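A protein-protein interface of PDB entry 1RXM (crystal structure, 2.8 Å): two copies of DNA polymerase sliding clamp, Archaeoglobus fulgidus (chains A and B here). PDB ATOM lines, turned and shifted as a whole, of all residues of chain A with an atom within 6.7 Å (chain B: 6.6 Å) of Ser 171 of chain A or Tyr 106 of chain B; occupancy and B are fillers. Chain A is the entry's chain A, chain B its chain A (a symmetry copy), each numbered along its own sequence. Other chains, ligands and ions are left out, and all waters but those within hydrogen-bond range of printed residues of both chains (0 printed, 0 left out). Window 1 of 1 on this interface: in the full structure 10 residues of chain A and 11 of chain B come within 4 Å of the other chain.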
ATOM      1  N   ILE A 148     -14.095  19.972  32.856  1.00  0.00           N
ATOM      2  CA  ILE A 148     -14.641  20.166  31.517  1.00  0.00           C
ATOM      3  C   ILE A 148     -15.726  21.231  31.397  1.00  0.00           C
ATOM      4  O   ILE A 148     -15.644  22.109  30.538  1.00  0.00           O
ATOM      5  CB  ILE A 148     -15.204  18.833  30.951  1.00  0.00           C
ATOM      6  CG1 ILE A 148     -14.057  17.866  30.648  1.00  0.00           C
ATOM      7  CG2 ILE A 148     -16.025  19.089  29.688  1.00  0.00           C
ATOM      8  CD1 ILE A 148     -13.420  17.248  31.878  1.00  0.00           C
ATOM      9  N   ALA A 165     -20.207  15.636  30.870  1.00  0.00           N
ATOM     10  CA  ALA A 165     -19.925  17.061  30.787  1.00  0.00           C
ATOM     11  C   ALA A 165     -19.401  17.320  29.386  1.00  0.00           C
ATOM     12  O   ALA A 165     -18.745  16.459  28.800  1.00  0.00           O
ATOM     13  CB  ALA A 165     -18.885  17.454  31.825  1.00  0.00           C
ATOM     14  N   LYS A 166     -19.690  18.493  28.838  1.00  0.00           N
ATOM     15  CA  LYS A 166     -19.229  18.815  27.495  1.00  0.00           C
ATOM     16  C   LYS A 166     -18.531  20.158  27.403  1.00  0.00           C
ATOM     17  O   LYS A 166     -19.030  21.162  27.908  1.00  0.00           O
ATOM     18  CB  LYS A 166     -20.398  18.788  26.503  1.00  0.00           C
ATOM     19  CG  LYS A 166     -20.946  17.392  26.231  1.00  0.00           C
ATOM     20  CD  LYS A 166     -22.461  17.311  26.422  1.00  0.00           C
ATOM     21  CE  LYS A 166     -22.933  15.853  26.529  1.00  0.00           C
ATOM     22  NZ  LYS A 166     -24.397  15.742  26.823  1.00  0.00           N
ATOM     23  N   GLY A 167     -17.366  20.154  26.760  1.00  0.00           N
ATOM     24  CA  GLY A 167     -16.604  21.370  26.557  1.00  0.00           C
ATOM     25  C   GLY A 167     -16.738  21.669  25.078  1.00  0.00           C
ATOM     26  O   GLY A 167     -17.451  20.959  24.378  1.00  0.00           O
ATOM     27  N   ASP A 168     -16.073  22.703  24.583  1.00  0.00           N
ATOM     28  CA  ASP A 168     -16.175  23.025  23.160  1.00  0.00           C
ATOM     29  C   ASP A 168     -15.116  22.307  22.326  1.00  0.00           C
ATOM     30  O   ASP A 168     -15.122  22.389  21.094  1.00  0.00           O
ATOM     31  CB  ASP A 168     -16.068  24.540  22.947  1.00  0.00           C
ATOM     32  CG  ASP A 168     -17.426  25.195  22.726  1.00  0.00           C
ATOM     33  OD1 ASP A 168     -18.127  24.790  21.768  1.00  0.00           O
ATOM     34  OD2 ASP A 168     -17.793  26.106  23.504  1.00  0.00           O
ATOM     35  N   VAL A 169     -14.227  21.587  23.005  1.00  0.00           N
ATOM     36  CA  VAL A 169     -13.143  20.871  22.346  1.00  0.00           C
ATOM     37  C   VAL A 169     -13.057  19.426  22.821  1.00  0.00           C
ATOM     38  O   VAL A 169     -12.462  18.570  22.156  1.00  0.00           O
ATOM     39  CB  VAL A 169     -11.800  21.600  22.611  1.00  0.00           C
ATOM     40  CG1 VAL A 169     -10.624  20.663  22.430  1.00  0.00           C
ATOM     41  CG2 VAL A 169     -11.679  22.795  21.673  1.00  0.00           C
ATOM     42  N   ASP A 170     -13.666  19.145  23.963  1.00  0.00           N
ATOM     43  CA  ASP A 170     -13.619  17.801  24.513  1.00  0.00           C
ATOM     44  C   ASP A 170     -14.813  17.519  25.410  1.00  0.00           C
ATOM     45  O   ASP A 170     -15.645  18.388  25.647  1.00  0.00           O
ATOM     46  CB  ASP A 170     -12.322  17.634  25.301  1.00  0.00           C
ATOM     47  CG  ASP A 170     -12.117  18.744  26.308  1.00  0.00           C
ATOM     48  OD1 ASP A 170     -11.021  18.834  26.900  1.00  0.00           O
ATOM     49  OD2 ASP A 170     -13.058  19.533  26.512  1.00  0.00           O
ATOM     50  N   SER A 171     -14.898  16.297  25.906  1.00  0.00           N
ATOM     51  CA  SER A 171     -15.987  15.930  26.788  1.00  0.00           C
ATOM     52  C   SER A 171     -15.555  14.773  27.676  1.00  0.00           C
ATOM     53  O   SER A 171     -14.518  14.151  27.449  1.00  0.00           O
ATOM     54  CB  SER A 171     -17.203  15.520  25.974  1.00  0.00           C
ATOM     55  OG  SER A 171     -16.902  14.360  25.225  1.00  0.00           O
ATOM     56  N   ILE A 172     -16.356  14.487  28.692  1.00  0.00           N
ATOM     57  CA  ILE A 172     -16.043  13.402  29.596  1.00  0.00           C
ATOM     58  C   ILE A 172     -17.345  12.726  29.978  1.00  0.00           C
ATOM     59  O   ILE A 172     -18.385  13.384  30.069  1.00  0.00           O
ATOM     60  CB  ILE A 172     -15.322  13.921  30.862  1.00  0.00           C
ATOM     61  CG1 ILE A 172     -14.643  12.764  31.586  1.00  0.00           C
ATOM     62  CG2 ILE A 172     -16.309  14.573  31.808  1.00  0.00           C
ATOM     63  CD1 ILE A 172     -13.648  13.223  32.637  1.00  0.00           C
ATOM     64  N   VAL A 173     -17.287  11.413  30.180  1.00  0.00           N
ATOM     65  CA  VAL A 173     -18.462  10.641  30.553  1.00  0.00           C
ATOM     66  C   VAL A 173     -18.136   9.567  31.584  1.00  0.00           C
ATOM     67  O   VAL A 173     -17.205   8.792  31.425  1.00  0.00           O
ATOM     68  CB  VAL A 173     -19.101   9.974  29.309  1.00  0.00           C
ATOM     69  CG1 VAL A 173     -20.136   8.936  29.724  1.00  0.00           C
ATOM     70  CG2 VAL A 173     -19.746  11.035  28.439  1.00  0.00           C
ATOM     71  N   ASP B  70      -3.238  18.328  22.445  1.00  0.00           N
ATOM     72  CA  ASP B  70      -3.311  19.539  23.263  1.00  0.00           C
ATOM     73  C   ASP B  70      -2.814  19.034  24.622  1.00  0.00           C
ATOM     74  O   ASP B  70      -3.573  18.448  25.400  1.00  0.00           O
ATOM     75  CB  ASP B  70      -4.760  20.026  23.385  1.00  0.00           C
ATOM     76  CG  ASP B  70      -4.882  21.359  24.132  1.00  0.00           C
ATOM     77  OD1 ASP B  70      -4.051  21.647  25.024  1.00  0.00           O
ATOM     78  OD2 ASP B  70      -5.829  22.118  23.831  1.00  0.00           O
ATOM     79  N   ARG B  73      -4.381  20.167  27.904  1.00  0.00           N
ATOM     80  CA  ARG B  73      -5.602  19.429  28.178  1.00  0.00           C
ATOM     81  C   ARG B  73      -5.344  18.033  28.740  1.00  0.00           C
ATOM     82  O   ARG B  73      -5.978  17.627  29.712  1.00  0.00           O
ATOM     83  CB  ARG B  73      -6.454  19.348  26.914  1.00  0.00           C
ATOM     84  CG  ARG B  73      -7.252  20.608  26.644  1.00  0.00           C
ATOM     85  CD  ARG B  73      -8.149  20.448  25.426  1.00  0.00           C
ATOM     86  NE  ARG B  73      -9.220  21.443  25.400  1.00  0.00           N
ATOM     87  CZ  ARG B  73      -9.023  22.757  25.314  1.00  0.00           C
ATOM     88  NH1 ARG B  73      -7.792  23.253  25.238  1.00  0.00           N
ATOM     89  NH2 ARG B  73     -10.061  23.581  25.315  1.00  0.00           N
ATOM     90  N   ILE B  74      -4.413  17.302  28.137  1.00  0.00           N
ATOM     91  CA  ILE B  74      -4.087  15.954  28.604  1.00  0.00           C
ATOM     92  C   ILE B  74      -3.500  16.028  30.010  1.00  0.00           C
ATOM     93  O   ILE B  74      -3.774  15.183  30.854  1.00  0.00           O
ATOM     94  CB  ILE B  74      -3.083  15.252  27.641  1.00  0.00           C
ATOM     95  CG1 ILE B  74      -3.707  15.134  26.255  1.00  0.00           C
ATOM     96  CG2 ILE B  74      -2.764  13.853  28.116  1.00  0.00           C
ATOM     97  CD1 ILE B  74      -5.044  14.415  26.257  1.00  0.00           C
ATOM     98  N   ILE B  77      -6.223  16.644  32.518  1.00  0.00           N
ATOM     99  CA  ILE B  77      -7.000  15.438  32.739  1.00  0.00           C
ATOM    100  C   ILE B  77      -6.266  14.364  33.537  1.00  0.00           C
ATOM    101  O   ILE B  77      -6.885  13.676  34.356  1.00  0.00           O
ATOM    102  CB  ILE B  77      -7.501  14.839  31.390  1.00  0.00           C
ATOM    103  CG1 ILE B  77      -8.981  15.158  31.213  1.00  0.00           C
ATOM    104  CG2 ILE B  77      -7.340  13.327  31.362  1.00  0.00           C
ATOM    105  CD1 ILE B  77      -9.860  14.573  32.307  1.00  0.00           C
ATOM    106  N   LEU B  97      -9.167  11.843  20.442  1.00  0.00           N
ATOM    107  CA  LEU B  97      -8.401  10.953  21.307  1.00  0.00           C
ATOM    108  C   LEU B  97      -9.213  10.544  22.535  1.00  0.00           C
ATOM    109  O   LEU B  97      -9.761  11.396  23.238  1.00  0.00           O
ATOM    110  CB  LEU B  97      -7.119  11.644  21.768  1.00  0.00           C
ATOM    111  CG  LEU B  97      -6.460  10.947  22.961  1.00  0.00           C
ATOM    112  CD1 LEU B  97      -6.091   9.532  22.558  1.00  0.00           C
ATOM    113  CD2 LEU B  97      -5.238  11.725  23.431  1.00  0.00           C
ATOM    114  N   LYS B  98      -9.285   9.240  22.788  1.00  0.00           N
ATOM    115  CA  LYS B  98     -10.019   8.720  23.941  1.00  0.00           C
ATOM    116  C   LYS B  98      -9.079   8.305  25.068  1.00  0.00           C
ATOM    117  O   LYS B  98      -8.115   7.571  24.846  1.00  0.00           O
ATOM    118  CB  LYS B  98     -10.864   7.506  23.553  1.00  0.00           C
ATOM    119  CG  LYS B  98     -12.064   7.791  22.682  1.00  0.00           C
ATOM    120  CD  LYS B  98     -12.921   6.539  22.591  1.00  0.00           C
ATOM    121  CE  LYS B  98     -14.191   6.756  21.782  1.00  0.00           C
ATOM    122  NZ  LYS B  98     -15.060   5.538  21.827  1.00  0.00           N
ATOM    123  N   VAL B  99      -9.377   8.764  26.279  1.00  0.00           N
ATOM    124  CA  VAL B  99      -8.565   8.427  27.440  1.00  0.00           C
ATOM    125  C   VAL B  99      -9.445   7.738  28.486  1.00  0.00           C
ATOM    126  O   VAL B  99     -10.327   8.362  29.066  1.00  0.00           O
ATOM    127  CB  VAL B  99      -7.927   9.691  28.051  1.00  0.00           C
ATOM    128  CG1 VAL B  99      -7.013   9.313  29.203  1.00  0.00           C
ATOM    129  CG2 VAL B  99      -7.158  10.442  26.980  1.00  0.00           C
ATOM    130  N   LYS B 100      -9.195   6.451  28.723  1.00  0.00           N
ATOM    131  CA  LYS B 100      -9.978   5.674  29.681  1.00  0.00           C
ATOM    132  C   LYS B 100      -9.275   5.259  30.963  1.00  0.00           C
ATOM    133  O   LYS B 100      -8.148   4.770  30.945  1.00  0.00           O
ATOM    134  CB  LYS B 100     -10.504   4.403  29.027  1.00  0.00           C
ATOM    135  CG  LYS B 100     -11.659   4.592  28.080  1.00  0.00           C
ATOM    136  CD  LYS B 100     -12.081   3.235  27.550  1.00  0.00           C
ATOM    137  CE  LYS B 100     -13.356   3.306  26.746  1.00  0.00           C
ATOM    138  NZ  LYS B 100     -13.725   1.935  26.309  1.00  0.00           N
ATOM    139  N   PHE B 101      -9.980   5.432  32.075  1.00  0.00           N
ATOM    140  CA  PHE B 101      -9.486   5.051  33.389  1.00  0.00           C
ATOM    141  C   PHE B 101     -10.688   5.078  34.319  1.00  0.00           C
ATOM    142  O   PHE B 101     -11.577   5.913  34.163  1.00  0.00           O
ATOM    143  CB  PHE B 101      -8.406   6.022  33.854  1.00  0.00           C
ATOM    144  CG  PHE B 101      -8.876   7.433  33.977  1.00  0.00           C
ATOM    145  CD1 PHE B 101      -9.357   7.915  35.190  1.00  0.00           C
ATOM    146  CD2 PHE B 101      -8.846   8.282  32.882  1.00  0.00           C
ATOM    147  CE1 PHE B 101      -9.796   9.221  35.314  1.00  0.00           C
ATOM    148  CE2 PHE B 101      -9.287   9.598  32.996  1.00  0.00           C
ATOM    149  CZ  PHE B 101      -9.762  10.067  34.218  1.00  0.00           C
ATOM    150  N   VAL B 104     -14.594   6.220  33.743  1.00  0.00           N
ATOM    151  CA  VAL B 104     -14.626   7.452  32.975  1.00  0.00           C
ATOM    152  C   VAL B 104     -14.030   7.315  31.573  1.00  0.00           C
ATOM    153  O   VAL B 104     -13.067   6.584  31.349  1.00  0.00           O
ATOM    154  CB  VAL B 104     -13.846   8.569  33.725  1.00  0.00           C
ATOM    155  CG1 VAL B 104     -13.719   9.804  32.852  1.00  0.00           C
ATOM    156  CG2 VAL B 104     -14.548   8.907  35.022  1.00  0.00           C
ATOM    157  N   GLU B 105     -14.625   8.024  30.624  1.00  0.00           N
ATOM    158  CA  GLU B 105     -14.129   8.041  29.260  1.00  0.00           C
ATOM    159  C   GLU B 105     -14.035   9.505  28.887  1.00  0.00           C
ATOM    160  O   GLU B 105     -15.028  10.229  28.929  1.00  0.00           O
ATOM    161  CB  GLU B 105     -15.075   7.324  28.296  1.00  0.00           C
ATOM    162  CG  GLU B 105     -14.570   7.347  26.858  1.00  0.00           C
ATOM    163  CD  GLU B 105     -15.345   6.421  25.941  1.00  0.00           C
ATOM    164  OE1 GLU B 105     -15.122   6.468  24.710  1.00  0.00           O
ATOM    165  OE2 GLU B 105     -16.175   5.637  26.455  1.00  0.00           O
ATOM    166  N   TYR B 106     -12.830   9.931  28.538  1.00  0.00           N
ATOM    167  CA  TYR B 106     -12.567  11.305  28.158  1.00  0.00           C
ATOM    168  C   TYR B 106     -12.230  11.357  26.675  1.00  0.00           C
ATOM    169  O   TYR B 106     -11.399  10.586  26.202  1.00  0.00           O
ATOM    170  CB  TYR B 106     -11.389  11.824  28.979  1.00  0.00           C
ATOM    171  CG  TYR B 106     -10.863  13.163  28.546  1.00  0.00           C
ATOM    172  CD1 TYR B 106     -11.528  14.344  28.883  1.00  0.00           C
ATOM    173  CD2 TYR B 106      -9.689  13.254  27.810  1.00  0.00           C
ATOM    174  CE1 TYR B 106     -11.025  15.587  28.493  1.00  0.00           C
ATOM    175  CE2 TYR B 106      -9.179  14.482  27.418  1.00  0.00           C
ATOM    176  CZ  TYR B 106      -9.844  15.643  27.762  1.00  0.00           C
ATOM    177  OH  TYR B 106      -9.302  16.849  27.398  1.00  0.00           O
ATOM    178  N   LYS B 107     -12.884  12.251  25.940  1.00  0.00           N
ATOM    179  CA  LYS B 107     -12.620  12.396  24.509  1.00  0.00           C
ATOM    180  C   LYS B 107     -12.131  13.810  24.216  1.00  0.00           C
ATOM    181  O   LYS B 107     -12.555  14.766  24.864  1.00  0.00           O
ATOM    182  CB  LYS B 107     -13.875  12.098  23.681  1.00  0.00           C
ATOM    183  CG  LYS B 107     -14.363  10.651  23.773  1.00  0.00           C
ATOM    184  CD  LYS B 107     -15.127  10.225  22.515  1.00  0.00           C
ATOM    185  CE  LYS B 107     -16.397  11.039  22.274  1.00  0.00           C
ATOM    186  NZ  LYS B 107     -17.479  10.738  23.265  1.00  0.00           N
ATOM    187  N   VAL B 108     -11.229  13.947  23.250  1.00  0.00           N
ATOM    188  CA  VAL B 108     -10.698  15.263  22.916  1.00  0.00           C
ATOM    189  C   VAL B 108     -10.288  15.359  21.452  1.00  0.00           C
ATOM    190  O   VAL B 108      -9.740  14.422  20.873  1.00  0.00           O
ATOM    191  CB  VAL B 108      -9.477  15.629  23.828  1.00  0.00           C
ATOM    192  CG1 VAL B 108      -8.319  14.662  23.587  1.00  0.00           C
ATOM    193  CG2 VAL B 108      -9.038  17.061  23.571  1.00  0.00           C
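N of Ala 165 of chain A sits at hydrogen-bond distance from O of Ile 172 of chain A, at 3.0 Å. NH1 of Arg 73 of chain B is in salt-bridge range of OD2 of Asp 70 of chain B, at 2.7 Å. The backbone NH (N) of Leu 97 of chain B sits at hydrogen-bond distance from the backbone carbonyl oxygen (O) of Val 108 of chain B. NZ of Lys 98 of chain B lies within salt-bridge range of OE1 of Glu 105 of chain B (3.0 Å). The backbone NH (N) of Val 99 of chain B is in hydrogen-bond range of the backbone carbonyl oxygen (O) of Tyr 106 of chain B, at 2.7 Å.
Among the printed residues, pairs that only touch across the chains: Val 169 of chain A with Arg 73 of chain B, Val 169 of chain A with Val 108 of chain B, Asp 170 of chain A with Lys 107 of chain B, Asp 170 of chain A with Val 108 of chain B, Ser 171 of chain A with Tyr 106 of chain B, Ile 172 of chain A with Val 104 of chain B, Ile 172 of chain A with Glu 105 of chain B and Val 173 of chain A with Val 104 of chain B.
Ser 171 of chain A touches just these residues of chain B: Tyr 106 (3.3 Å) and Lys 107 (2.9 Å). Of chain A, only Asp 170 (2.7 Å) and Ser 171 (3.3 Å) come within 4 Å of Tyr 106 of chain B. Of the printed residues of chain A, Val 104 of chain B touches Ile 172 and Val 173. Printed residues of chain B within 4 Å of Ile 172 of chain A: Val 104 (3.3 Å) and Glu 105 (3.4 Å). Leu 97 of chain B touches none of the printed residues of chain A. The nearest residue of chain B that does not touch Ser 171 of chain A is Glu 105 of chain B (4.2 Å). The nearest printed residue of chain A that does not touch Lys 107 of chain B is Val 169 of chain A (4.7 Å).
No position is printed for both chains. Of the 12 pairs that touch across the chains among the printed residues, none has its exchanged pair printed and touching as well.
The guanidinium group (NE) of Arg 73 of chain B is in salt-bridge range of the side-chain carboxylate (OD1) of Asp 170 of chain A. OD1 of Asp 170 of chain A lies within hydrogen-bond range of OH of Tyr 106 of chain B. O of Ser 171 of chain A sits at hydrogen-bond distance from N of Lys 107 of chain B, 2.9 Å away. The backbone carbonyl oxygen of Val 173 of chain A is in hydrogen-bond range of the backbone NH of Glu 105 of chain B (2.8 Å).
Printed residues of chain B that touch a printed residue of chain A: Arg 73, Val 104, Glu 105, Tyr 106, Lys 107 and Val 108. Of the 10 printed residues of chain A, 5 touch a printed residue of chain B. Printed residues of chain A that touch a printed residue of chain B: Val 169, Asp 170, Ser 171, Ile 172 and Val 173. Hydrophobic or aromatic side chains of chain A within 4 Å of the printed part of chain B: Val 169 and Ile 172. Among the printed residues, 12 pairs touch across the chains. Among the printed residues, Asp or Glu carboxylates within 4 Å of a Lys or Arg side-chain nitrogen of the other chain: Asp 170 of chain A with Arg 73 of chain B (3.5 Å).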
